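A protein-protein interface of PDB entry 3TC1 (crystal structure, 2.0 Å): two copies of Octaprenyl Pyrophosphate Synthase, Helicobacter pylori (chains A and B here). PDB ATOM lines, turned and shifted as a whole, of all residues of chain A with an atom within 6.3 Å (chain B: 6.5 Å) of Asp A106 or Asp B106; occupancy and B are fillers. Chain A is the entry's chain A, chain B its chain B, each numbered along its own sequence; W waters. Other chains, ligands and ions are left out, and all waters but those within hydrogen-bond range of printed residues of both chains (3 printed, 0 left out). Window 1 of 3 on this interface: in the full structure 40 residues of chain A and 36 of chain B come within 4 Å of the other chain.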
ATOM      1  N   ALA A  72      30.980  -7.421   2.696  1.00  0.00           N
ATOM      2  CA  ALA A  72      31.122  -6.275   1.805  1.00  0.00           C
ATOM      3  C   ALA A  72      31.313  -5.001   2.612  1.00  0.00           C
ATOM      4  O   ALA A  72      32.177  -4.180   2.301  1.00  0.00           O
ATOM      5  CB  ALA A  72      29.877  -6.140   0.899  1.00  0.00           C
ATOM      6  N   SER A  73      30.509  -4.830   3.655  1.00  0.00           N
ATOM      7  CA  SER A  73      30.617  -3.621   4.464  1.00  0.00           C
ATOM      8  C   SER A  73      31.949  -3.547   5.200  1.00  0.00           C
ATOM      9  O   SER A  73      32.506  -2.465   5.354  1.00  0.00           O
ATOM     10  CB  SER A  73      29.458  -3.517   5.461  1.00  0.00           C
ATOM     11  OG  SER A  73      29.610  -4.424   6.531  1.00  0.00           O
ATOM     12  N   LEU A  75      34.749  -4.783   4.150  1.00  0.00           N
ATOM     13  CA  LEU A  75      35.711  -4.428   3.114  1.00  0.00           C
ATOM     14  C   LEU A  75      35.735  -2.945   2.852  1.00  0.00           C
ATOM     15  O   LEU A  75      36.768  -2.304   2.839  1.00  0.00           O
ATOM     16  CB  LEU A  75      35.351  -5.160   1.829  1.00  0.00           C
ATOM     17  CG  LEU A  75      35.622  -6.682   1.908  1.00  0.00           C
ATOM     18  CD1 LEU A  75      34.989  -7.433   0.702  1.00  0.00           C
ATOM     19  CD2 LEU A  75      37.188  -6.904   2.041  1.00  0.00           C
ATOM     20  N   HIS A  76      34.562  -2.374   2.676  1.00  0.00           N
ATOM     21  CA  HIS A  76      34.501  -0.940   2.400  1.00  0.00           C
ATOM     22  C   HIS A  76      34.889  -0.118   3.581  1.00  0.00           C
ATOM     23  O   HIS A  76      35.403   0.993   3.481  1.00  0.00           O
ATOM     24  CB  HIS A  76      33.110  -0.541   1.889  1.00  0.00           C
ATOM     25  CG  HIS A  76      32.897  -0.981   0.480  1.00  0.00           C
ATOM     26  ND1 HIS A  76      31.821  -0.582  -0.291  1.00  0.00           N
ATOM     27  CD2 HIS A  76      33.674  -1.737  -0.320  1.00  0.00           C
ATOM     28  CE1 HIS A  76      31.964  -1.077  -1.511  1.00  0.00           C
ATOM     29  NE2 HIS A  76      33.088  -1.782  -1.548  1.00  0.00           N
ATOM     30  N   ALA A 101      40.031  -3.901  -2.105  1.00  0.00           N
ATOM     31  CA  ALA A 101      39.005  -3.981  -1.073  1.00  0.00           C
ATOM     32  C   ALA A 101      37.718  -3.320  -1.552  1.00  0.00           C
ATOM     33  O   ALA A 101      36.624  -3.822  -1.308  1.00  0.00           O
ATOM     34  CB  ALA A 101      39.492  -3.306   0.203  1.00  0.00           C
ATOM     35  N   VAL A 102      37.847  -2.185  -2.228  1.00  0.00           N
ATOM     36  CA  VAL A 102      36.673  -1.493  -2.733  1.00  0.00           C
ATOM     37  C   VAL A 102      36.034  -2.368  -3.804  1.00  0.00           C
ATOM     38  O   VAL A 102      34.809  -2.515  -3.854  1.00  0.00           O
ATOM     39  CB  VAL A 102      37.045  -0.124  -3.347  1.00  0.00           C
ATOM     40  CG1 VAL A 102      35.830   0.502  -4.006  1.00  0.00           C
ATOM     41  CG2 VAL A 102      37.586   0.801  -2.263  1.00  0.00           C
ATOM     42  N   MET A 103      36.877  -2.965  -4.646  1.00  0.00           N
ATOM     43  CA  MET A 103      36.405  -3.820  -5.731  1.00  0.00           C
ATOM     44  C   MET A 103      35.744  -5.103  -5.237  1.00  0.00           C
ATOM     45  O   MET A 103      34.651  -5.450  -5.674  1.00  0.00           O
ATOM     46  CB  MET A 103      37.562  -4.175  -6.675  1.00  0.00           C
ATOM     47  CG  MET A 103      38.229  -2.978  -7.333  1.00  0.00           C
ATOM     48  SD  MET A 103      39.358  -3.438  -8.676  1.00  0.00           S
ATOM     49  CE  MET A 103      40.700  -4.261  -7.756  1.00  0.00           C
ATOM     50  N   LEU A 104      36.414  -5.818  -4.340  1.00  0.00           N
ATOM     51  CA  LEU A 104      35.855  -7.060  -3.824  1.00  0.00           C
ATOM     52  C   LEU A 104      34.562  -6.764  -3.066  1.00  0.00           C
ATOM     53  O   LEU A 104      33.643  -7.581  -3.049  1.00  0.00           O
ATOM     54  CB  LEU A 104      36.862  -7.762  -2.911  1.00  0.00           C
ATOM     55  CG  LEU A 104      36.487  -9.196  -2.524  1.00  0.00           C
ATOM     56  CD1 LEU A 104      36.337 -10.045  -3.781  1.00  0.00           C
ATOM     57  CD2 LEU A 104      37.549  -9.776  -1.608  1.00  0.00           C
ATOM     58  N   GLY A 105      34.492  -5.584  -2.456  1.00  0.00           N
ATOM     59  CA  GLY A 105      33.304  -5.192  -1.718  1.00  0.00           C
ATOM     60  C   GLY A 105      32.101  -5.024  -2.627  1.00  0.00           C
ATOM     61  O   GLY A 105      30.977  -5.387  -2.266  1.00  0.00           O
ATOM     62  N   ASP A 106      32.335  -4.475  -3.817  1.00  0.00           N
ATOM     63  CA  ASP A 106      31.263  -4.276  -4.781  1.00  0.00           C
ATOM     64  C   ASP A 106      30.791  -5.617  -5.325  1.00  0.00           C
ATOM     65  O   ASP A 106      29.611  -5.791  -5.603  1.00  0.00           O
ATOM     66  CB  ASP A 106      31.725  -3.384  -5.939  1.00  0.00           C
ATOM     67  CG  ASP A 106      31.832  -1.927  -5.545  1.00  0.00           C
ATOM     68  OD1 ASP A 106      31.049  -1.486  -4.670  1.00  0.00           O
ATOM     69  OD2 ASP A 106      32.688  -1.220  -6.121  1.00  0.00           O
ATOM     70  N   VAL A 107      31.724  -6.554  -5.478  1.00  0.00           N
ATOM     71  CA  VAL A 107      31.410  -7.896  -5.965  1.00  0.00           C
ATOM     72  C   VAL A 107      30.488  -8.596  -4.961  1.00  0.00           C
ATOM     73  O   VAL A 107      29.488  -9.211  -5.337  1.00  0.00           O
ATOM     74  CB  VAL A 107      32.696  -8.743  -6.142  1.00  0.00           C
ATOM     75  CG1 VAL A 107      32.340 -10.211  -6.314  1.00  0.00           C
ATOM     76  CG2 VAL A 107      33.478  -8.259  -7.352  1.00  0.00           C
ATOM     77  N   PHE A 108      30.834  -8.503  -3.681  1.00  0.00           N
ATOM     78  CA  PHE A 108      30.025  -9.122  -2.637  1.00  0.00           C
ATOM     79  C   PHE A 108      28.638  -8.491  -2.573  1.00  0.00           C
ATOM     80  O   PHE A 108      27.636  -9.199  -2.527  1.00  0.00           O
ATOM     81  CB  PHE A 108      30.714  -9.004  -1.273  1.00  0.00           C
ATOM     82  CG  PHE A 108      31.609 -10.164  -0.940  1.00  0.00           C
ATOM     83  CD1 PHE A 108      32.855 -10.303  -1.544  1.00  0.00           C
ATOM     84  CD2 PHE A 108      31.200 -11.129  -0.019  1.00  0.00           C
ATOM     85  CE1 PHE A 108      33.682 -11.389  -1.233  1.00  0.00           C
ATOM     86  CE2 PHE A 108      32.014 -12.213   0.297  1.00  0.00           C
ATOM     87  CZ  PHE A 108      33.258 -12.345  -0.309  1.00  0.00           C
ATOM     88  N   TYR A 109      28.578  -7.163  -2.575  1.00  0.00           N
ATOM     89  CA  TYR A 109      27.299  -6.459  -2.525  1.00  0.00           C
ATOM     90  C   TYR A 109      26.405  -6.803  -3.717  1.00  0.00           C
ATOM     91  O   TYR A 109      25.219  -7.102  -3.551  1.00  0.00           O
ATOM     92  CB  TYR A 109      27.507  -4.938  -2.512  1.00  0.00           C
ATOM     93  CG  TYR A 109      27.667  -4.302  -1.145  1.00  0.00           C
ATOM     94  CD1 TYR A 109      26.805  -4.620  -0.095  1.00  0.00           C
ATOM     95  CD2 TYR A 109      28.645  -3.330  -0.921  1.00  0.00           C
ATOM     96  CE1 TYR A 109      26.911  -3.979   1.149  1.00  0.00           C
ATOM     97  CE2 TYR A 109      28.760  -2.683   0.319  1.00  0.00           C
ATOM     98  CZ  TYR A 109      27.893  -3.008   1.343  1.00  0.00           C
ATOM     99  OH  TYR A 109      27.996  -2.365   2.558  1.00  0.00           O
ATOM    100  N   SER A 110      26.973  -6.746  -4.920  1.00  0.00           N
ATOM    101  CA  SER A 110      26.202  -7.018  -6.127  1.00  0.00           C
ATOM    102  C   SER A 110      25.702  -8.460  -6.238  1.00  0.00           C
ATOM    103  O   SER A 110      24.556  -8.690  -6.616  1.00  0.00           O
ATOM    104  CB  SER A 110      27.013  -6.620  -7.370  1.00  0.00           C
ATOM    105  OG  SER A 110      28.260  -7.281  -7.419  1.00  0.00           O
ATOM    106  N   LYS A 111      26.543  -9.433  -5.906  1.00  0.00           N
ATOM    107  CA  LYS A 111      26.108 -10.831  -5.977  1.00  0.00           C
ATOM    108  C   LYS A 111      24.998 -11.062  -4.953  1.00  0.00           C
ATOM    109  O   LYS A 111      23.970 -11.685  -5.255  1.00  0.00           O
ATOM    110  CB  LYS A 111      27.287 -11.769  -5.712  1.00  0.00           C
ATOM    111  CG  LYS A 111      26.934 -13.265  -5.664  1.00  0.00           C
ATOM    112  CD  LYS A 111      26.283 -13.776  -6.960  1.00  0.00           C
ATOM    113  CE  LYS A 111      26.065 -15.286  -6.900  1.00  0.00           C
ATOM    114  NZ  LYS A 111      25.387 -15.850  -8.106  1.00  0.00           N
ATOM    115  N   VAL A 131      21.348  -1.828   4.164  1.00  0.00           N
ATOM    116  CA  VAL A 131      22.635  -1.458   3.581  1.00  0.00           C
ATOM    117  C   VAL A 131      22.691   0.051   3.409  1.00  0.00           C
ATOM    118  O   VAL A 131      23.738   0.672   3.604  1.00  0.00           O
ATOM    119  CB  VAL A 131      22.866  -2.137   2.216  1.00  0.00           C
ATOM    120  CG1 VAL A 131      24.131  -1.581   1.562  1.00  0.00           C
ATOM    121  CG2 VAL A 131      22.996  -3.644   2.404  1.00  0.00           C
ATOM    122  N   LEU A 132      21.557   0.643   3.055  1.00  0.00           N
ATOM    123  CA  LEU A 132      21.488   2.084   2.892  1.00  0.00           C
ATOM    124  C   LEU A 132      21.771   2.754   4.230  1.00  0.00           C
ATOM    125  O   LEU A 132      22.548   3.703   4.316  1.00  0.00           O
ATOM    126  CB  LEU A 132      20.101   2.507   2.402  1.00  0.00           C
ATOM    127  CG  LEU A 132      19.848   4.020   2.358  1.00  0.00           C
ATOM    128  CD1 LEU A 132      20.889   4.698   1.477  1.00  0.00           C
ATOM    129  CD2 LEU A 132      18.443   4.287   1.840  1.00  0.00           C
ATOM    130  N   SER A 135      25.392   2.439   5.411  1.00  0.00           N
ATOM    131  CA  SER A 135      26.289   3.275   4.624  1.00  0.00           C
ATOM    132  C   SER A 135      26.127   4.713   5.121  1.00  0.00           C
ATOM    133  O   SER A 135      27.092   5.475   5.185  1.00  0.00           O
ATOM    134  CB  SER A 135      25.960   3.160   3.136  1.00  0.00           C
ATOM    135  OG  SER A 135      26.277   1.856   2.676  1.00  0.00           O
ATOM    136  N   ALA B  72      27.029   5.724  -9.104  1.00  0.00           N
ATOM    137  CA  ALA B  72      27.732   4.969  -8.070  1.00  0.00           C
ATOM    138  C   ALA B  72      29.001   4.341  -8.634  1.00  0.00           C
ATOM    139  O   ALA B  72      30.060   4.377  -8.001  1.00  0.00           O
ATOM    140  CB  ALA B  72      26.825   3.878  -7.487  1.00  0.00           C
ATOM    141  N   LEU B  75      31.668   6.903  -9.091  1.00  0.00           N
ATOM    142  CA  LEU B  75      32.226   7.308  -7.805  1.00  0.00           C
ATOM    143  C   LEU B  75      33.293   6.320  -7.359  1.00  0.00           C
ATOM    144  O   LEU B  75      34.359   6.720  -6.900  1.00  0.00           O
ATOM    145  CB  LEU B  75      31.131   7.389  -6.741  1.00  0.00           C
ATOM    146  CG  LEU B  75      30.142   8.557  -6.825  1.00  0.00           C
ATOM    147  CD1 LEU B  75      29.062   8.367  -5.762  1.00  0.00           C
ATOM    148  CD2 LEU B  75      30.866   9.888  -6.621  1.00  0.00           C
ATOM    149  N   HIS B  76      33.012   5.027  -7.489  1.00  0.00           N
ATOM    150  CA  HIS B  76      33.986   4.020  -7.091  1.00  0.00           C
ATOM    151  C   HIS B  76      35.152   3.963  -8.066  1.00  0.00           C
ATOM    152  O   HIS B  76      36.290   3.742  -7.659  1.00  0.00           O
ATOM    153  CB  HIS B  76      33.328   2.638  -6.964  1.00  0.00           C
ATOM    154  CG  HIS B  76      32.514   2.477  -5.715  1.00  0.00           C
ATOM    155  ND1 HIS B  76      31.894   1.295  -5.372  1.00  0.00           N
ATOM    156  CD2 HIS B  76      32.211   3.358  -4.733  1.00  0.00           C
ATOM    157  CE1 HIS B  76      31.239   1.456  -4.236  1.00  0.00           C
ATOM    158  NE2 HIS B  76      31.415   2.699  -3.828  1.00  0.00           N
ATOM    159  N   ALA B 101      33.811   8.861  -0.755  1.00  0.00           N
ATOM    160  CA  ALA B 101      33.452   8.593  -2.143  1.00  0.00           C
ATOM    161  C   ALA B 101      32.960   7.154  -2.264  1.00  0.00           C
ATOM    162  O   ALA B 101      32.015   6.874  -2.998  1.00  0.00           O
ATOM    163  CB  ALA B 101      34.651   8.819  -3.056  1.00  0.00           C
ATOM    164  N   VAL B 102      33.600   6.248  -1.532  1.00  0.00           N
ATOM    165  CA  VAL B 102      33.217   4.839  -1.559  1.00  0.00           C
ATOM    166  C   VAL B 102      31.852   4.645  -0.902  1.00  0.00           C
ATOM    167  O   VAL B 102      30.973   4.004  -1.474  1.00  0.00           O
ATOM    168  CB  VAL B 102      34.252   3.944  -0.830  1.00  0.00           C
ATOM    169  CG1 VAL B 102      33.769   2.499  -0.805  1.00  0.00           C
ATOM    170  CG2 VAL B 102      35.591   4.020  -1.539  1.00  0.00           C
ATOM    171  N   MET B 103      31.679   5.195   0.298  1.00  0.00           N
ATOM    172  CA  MET B 103      30.405   5.070   1.000  1.00  0.00           C
ATOM    173  C   MET B 103      29.278   5.736   0.221  1.00  0.00           C
ATOM    174  O   MET B 103      28.171   5.203   0.157  1.00  0.00           O
ATOM    175  CB  MET B 103      30.478   5.684   2.402  1.00  0.00           C
ATOM    176  CG  MET B 103      31.260   4.869   3.420  1.00  0.00           C
ATOM    177  SD  MET B 103      30.683   3.159   3.575  1.00  0.00           S
ATOM    178  CE  MET B 103      32.201   2.296   3.352  1.00  0.00           C
ATOM    179  N   LEU B 104      29.554   6.902  -0.359  1.00  0.00           N
ATOM    180  CA  LEU B 104      28.543   7.613  -1.134  1.00  0.00           C
ATOM    181  C   LEU B 104      28.096   6.749  -2.310  1.00  0.00           C
ATOM    182  O   LEU B 104      26.934   6.767  -2.694  1.00  0.00           O
ATOM    183  CB  LEU B 104      29.083   8.948  -1.652  1.00  0.00           C
ATOM    184  CG  LEU B 104      28.064   9.742  -2.484  1.00  0.00           C
ATOM    185  CD1 LEU B 104      26.886  10.148  -1.611  1.00  0.00           C
ATOM    186  CD2 LEU B 104      28.721  10.966  -3.097  1.00  0.00           C
ATOM    187  N   GLY B 105      29.031   5.995  -2.877  1.00  0.00           N
ATOM    188  CA  GLY B 105      28.697   5.111  -3.977  1.00  0.00           C
ATOM    189  C   GLY B 105      27.823   3.975  -3.472  1.00  0.00           C
ATOM    190  O   GLY B 105      26.901   3.527  -4.155  1.00  0.00           O
ATOM    191  N   ASP B 106      28.112   3.505  -2.261  1.00  0.00           N
ATOM    192  CA  ASP B 106      27.333   2.420  -1.666  1.00  0.00           C
ATOM    193  C   ASP B 106      25.918   2.903  -1.390  1.00  0.00           C
ATOM    194  O   ASP B 106      24.953   2.147  -1.513  1.00  0.00           O
ATOM    195  CB  ASP B 106      27.979   1.939  -0.361  1.00  0.00           C
ATOM    196  CG  ASP B 106      29.246   1.148  -0.603  1.00  0.00           C
ATOM    197  OD1 ASP B 106      29.469   0.730  -1.762  1.00  0.00           O
ATOM    198  OD2 ASP B 106      30.006   0.931   0.364  1.00  0.00           O
ATOM    199  N   VAL B 107      25.819   4.168  -0.999  1.00  0.00           N
ATOM    200  CA  VAL B 107      24.539   4.814  -0.729  1.00  0.00           C
ATOM    201  C   VAL B 107      23.729   4.880  -2.027  1.00  0.00           C
ATOM    202  O   VAL B 107      22.537   4.575  -2.044  1.00  0.00           O
ATOM    203  CB  VAL B 107      24.752   6.247  -0.202  1.00  0.00           C
ATOM    204  CG1 VAL B 107      23.466   7.055  -0.343  1.00  0.00           C
ATOM    205  CG2 VAL B 107      25.194   6.204   1.264  1.00  0.00           C
ATOM    206  N   PHE B 108      24.379   5.288  -3.116  1.00  0.00           N
ATOM    207  CA  PHE B 108      23.693   5.363  -4.400  1.00  0.00           C
ATOM    208  C   PHE B 108      23.223   3.974  -4.809  1.00  0.00           C
ATOM    209  O   PHE B 108      22.071   3.803  -5.209  1.00  0.00           O
ATOM    210  CB  PHE B 108      24.606   5.948  -5.485  1.00  0.00           C
ATOM    211  CG  PHE B 108      24.436   7.434  -5.691  1.00  0.00           C
ATOM    212  CD1 PHE B 108      24.924   8.343  -4.758  1.00  0.00           C
ATOM    213  CD2 PHE B 108      23.785   7.920  -6.822  1.00  0.00           C
ATOM    214  CE1 PHE B 108      24.770   9.718  -4.948  1.00  0.00           C
ATOM    215  CE2 PHE B 108      23.623   9.290  -7.026  1.00  0.00           C
ATOM    216  CZ  PHE B 108      24.118  10.195  -6.084  1.00  0.00           C
ATOM    217  N   TYR B 109      24.108   2.986  -4.699  1.00  0.00           N
ATOM    218  CA  TYR B 109      23.773   1.607  -5.050  1.00  0.00           C
ATOM    219  C   TYR B 109      22.620   1.036  -4.222  1.00  0.00           C
ATOM    220  O   TYR B 109      21.698   0.441  -4.770  1.00  0.00           O
ATOM    221  CB  TYR B 109      24.979   0.680  -4.864  1.00  0.00           C
ATOM    222  CG  TYR B 109      25.962   0.639  -6.013  1.00  0.00           C
ATOM    223  CD1 TYR B 109      25.525   0.480  -7.331  1.00  0.00           C
ATOM    224  CD2 TYR B 109      27.339   0.705  -5.778  1.00  0.00           C
ATOM    225  CE1 TYR B 109      26.434   0.387  -8.386  1.00  0.00           C
ATOM    226  CE2 TYR B 109      28.256   0.610  -6.825  1.00  0.00           C
ATOM    227  CZ  TYR B 109      27.796   0.454  -8.126  1.00  0.00           C
ATOM    228  OH  TYR B 109      28.696   0.372  -9.162  1.00  0.00           O
ATOM    229  N   SER B 110      22.682   1.197  -2.902  1.00  0.00           N
ATOM    230  CA  SER B 110      21.638   0.650  -2.034  1.00  0.00           C
ATOM    231  C   SER B 110      20.286   1.354  -2.181  1.00  0.00           C
ATOM    232  O   SER B 110      19.246   0.696  -2.212  1.00  0.00           O
ATOM    233  CB  SER B 110      22.099   0.649  -0.567  1.00  0.00           C
ATOM    234  OG  SER B 110      22.582   1.914  -0.159  1.00  0.00           O
ATOM    235  N   LYS B 111      20.294   2.681  -2.281  1.00  0.00           N
ATOM    236  CA  LYS B 111      19.045   3.417  -2.452  1.00  0.00           C
ATOM    237  C   LYS B 111      18.431   2.998  -3.782  1.00  0.00           C
ATOM    238  O   LYS B 111      17.220   2.805  -3.883  1.00  0.00           O
ATOM    239  CB  LYS B 111      19.293   4.931  -2.438  1.00  0.00           C
ATOM    240  CG  LYS B 111      18.045   5.789  -2.722  1.00  0.00           C
ATOM    241  CD  LYS B 111      16.906   5.537  -1.723  1.00  0.00           C
ATOM    242  CE  LYS B 111      15.692   6.410  -2.038  1.00  0.00           C
ATOM    243  NZ  LYS B 111      14.513   6.147  -1.162  1.00  0.00           N
ATOM    244  N   VAL B 131      24.962  -4.919 -12.474  1.00  0.00           N
ATOM    245  CA  VAL B 131      25.857  -4.294 -11.506  1.00  0.00           C
ATOM    246  C   VAL B 131      26.939  -5.307 -11.102  1.00  0.00           C
ATOM    247  O   VAL B 131      28.078  -4.929 -10.842  1.00  0.00           O
ATOM    248  CB  VAL B 131      25.104  -3.811 -10.246  1.00  0.00           C
ATOM    249  CG1 VAL B 131      26.096  -3.245  -9.235  1.00  0.00           C
ATOM    250  CG2 VAL B 131      24.089  -2.733 -10.623  1.00  0.00           C
ATOM    251  N   LEU B 132      26.586  -6.588 -11.058  1.00  0.00           N
ATOM    252  CA  LEU B 132      27.559  -7.620 -10.712  1.00  0.00           C
ATOM    253  C   LEU B 132      28.622  -7.703 -11.808  1.00  0.00           C
ATOM    254  O   LEU B 132      29.804  -7.894 -11.530  1.00  0.00           O
ATOM    255  CB  LEU B 132      26.876  -8.980 -10.550  1.00  0.00           C
ATOM    256  CG  LEU B 132      27.810 -10.173 -10.303  1.00  0.00           C
ATOM    257  CD1 LEU B 132      28.648  -9.933  -9.053  1.00  0.00           C
ATOM    258  CD2 LEU B 132      26.993 -11.444 -10.161  1.00  0.00           C
ATOM    259  N   SER B 135      31.022  -4.751 -11.658  1.00  0.00           N
ATOM    260  CA  SER B 135      32.055  -4.922 -10.644  1.00  0.00           C
ATOM    261  C   SER B 135      33.109  -5.925 -11.108  1.00  0.00           C
ATOM    262  O   SER B 135      34.293  -5.760 -10.821  1.00  0.00           O
ATOM    263  CB  SER B 135      31.440  -5.358  -9.305  1.00  0.00           C
ATOM    264  OG  SER B 135      31.028  -6.717  -9.324  1.00  0.00           O
ATOM    265  N   GLU B 138      35.266  -4.092 -13.573  1.00  0.00           N
ATOM    266  CA  GLU B 138      36.161  -3.129 -12.950  1.00  0.00           C
ATOM    267  C   GLU B 138      37.404  -3.858 -12.437  1.00  0.00           C
ATOM    268  O   GLU B 138      38.526  -3.391 -12.622  1.00  0.00           O
ATOM    269  CB  GLU B 138      35.452  -2.414 -11.798  1.00  0.00           C
ATOM    270  CG  GLU B 138      36.349  -1.465 -11.024  1.00  0.00           C
ATOM    271  CD  GLU B 138      36.886  -0.325 -11.876  1.00  0.00           C
ATOM    272  OE1 GLU B 138      37.724   0.443 -11.360  1.00  0.00           O
ATOM    273  OE2 GLU B 138      36.472  -0.191 -13.049  1.00  0.00           O
HETATM  274  O   HOH W   1      28.786   0.197   2.793  1.00  0.00           O
HETATM  275  O   HOH W   2      34.733  -4.282  -8.564  1.00  0.00           O
HETATM  276  O   HOH W   3      31.138  -0.022  -8.537  1.00  0.00           O
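Asp A106 touches its own counterpart, Asp B106. Val A107 touches Leu B132, and with the chains exchanged Leu A132 touches Val B107. Val A107 touches Ser B135, and with the chains exchanged Ser A135 touches Val B107. Ser A110 touches Val B131, and with the chains exchanged Val A131 touches Ser B110. Positions printed for both chains: 72, 75, 76, 101, 102, 103, 104, 105, 106, 107, 108, 109, 110, 111, 131, 132 and 135.
The backbone carbonyl oxygen of Val A131 lies within hydrogen-bond range of the side-chain hydroxyl of Ser A135 (3.0 Å). The backbone carbonyl oxygen (O) of Asp A106 lies within hydrogen-bond range of the side-chain hydroxyl (OG) of Ser A110 (2.7 Å). The backbone carbonyl oxygen (O) of Asp B106 sits at hydrogen-bond distance from the side-chain hydroxyl (OG) of Ser B110 (2.7 Å). NE2 of His B76 lies within hydrogen-bond range of O of Val B102 (2.7 Å). A ring nitrogen (NE2) of His B76 sits close to the side-chain carboxylate (OD1) of Asp B106. A ring nitrogen (NE2) of His A76 is in hydrogen-bond range of the backbone carbonyl oxygen (O) of Val A102, 3.0 Å away.
Water W3 lies within hydrogen-bond range of the side-chain hydroxyl (OH) of Tyr B109 (2.6 Å) and the side-chain carboxylate (OD2) of Asp A106 (3.1 Å). Water W1 lies within hydrogen-bond range of the side-chain hydroxyl of Tyr A109 (2.7 Å), the side-chain carboxylate of Asp B106 (2.8 Å), the side-chain hydroxyl of Ser A135 (3.0 Å) and the side-chain sulfur of Met B103 (3.6 Å). Water W2 lies within hydrogen-bond range of the backbone carbonyl oxygen of Ser B135 (2.7 Å) and the backbone carbonyl oxygen of Met A103 (3.1 Å).
Of the 18 printed residues of chain B, 9 touch a printed residue of chain A. Hydrophobic or aromatic side chains of chain B within 4 Å of the printed part of chain A: His B76, Val B102, Met B103, Val B107, Val B131 and Leu B132. Of the 18 printed residues of chain A, 10 touch a printed residue of chain B. Printed residues of chain A that touch a printed residue of chain B: His A76, Val A102, Asp A106, Val A107, Tyr A109, Ser A110, Lys A111, Val A131, Leu A132 and Ser A135. Hydrophobic or aromatic side chains of chain A that line the printed part of chain B: His A76, Val A102, Val A107, Tyr A109, Val A131 and Leu A132. Among the printed residues, no Asp or Glu carboxylate lies within 4 Å of a Lys or Arg side-chain nitrogen of the other chain.
Among the printed residues, merely in contact across the chains: Ser A110 with Leu B132 (3.1 Å), Leu A132 with Ser B110 (3.2 Å), His A76 with Met B103 (3.3 Å), Ser A135 with Asp B106 (3.5 Å), Val A107 with Ser B135 (3.5 Å), Ser A135 with Val B107 (3.7 Å), His A76 with Val B102 (3.7 Å), Val A131 with Ser B110 (3.7 Å), His A76 with His B76 (3.8 Å), Lys A111 with Leu B132 (3.8 Å), Tyr A109 with Asp B106 (3.8 Å), Val A102 with Val B102 (3.9 Å), Val A107 with Leu B132 (3.9 Å), Leu A132 with Val B107 (3.9 Å), Asp A106 with Ser B135 (3.9 Å), Ser A110 with Val B131 (3.96 Å) and Asp A106 with Asp B106 (3.98 Å).
Printed residues of chain B within 4 Å of His A76: His B76 (3.8 Å), Val B102 (3.7 Å), Met B103 (3.3 Å) and Asp B106 (2.5 Å). Printed residues of chain B within 4 Å of Asp A106: His B76, Asp B106 and Ser B135. Printed residues of chain B within 4 Å of Ser A135: Asp B106 and Val B107. Of the printed residues of chain A, Val B102 touches His A76 and Val A102. Leu B104 touches none of the printed residues of chain A. Of the printed residues of chain A, Asp B106 touches His A76 (2.5 Å), Asp A106 (3.98 Å), Tyr A109 (3.8 Å) and Ser A135 (3.5 Å). Of the printed residues of chain A, Val B107 touches Leu A132 (3.9 Å) and Ser A135 (3.7 Å). Lys B111 touches none of the printed residues of chain A. Printed residues of chain A within 4 Å of Ser B135: Asp A106, Val A107 and Ser A110. The nearest printed residue of chain B that does not touch Asp A106 is Tyr B109 (4.1 Å). The nearest printed residue of chain A that does not touch Asp B106 is Val A131 (4.9 Å).
The side-chain hydroxyl of Ser A110 is in hydrogen-bond range of the side-chain hydroxyl of Ser B135 (3.4 Å). ND1 of His A76 lies within hydrogen-bond range of OD2 of Asp B106 (2.5 Å). A ring nitrogen (ND1) of His B76 is in hydrogen-bond range of the side-chain carboxylate (OD2) of Asp A106, at 2.7 Å.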
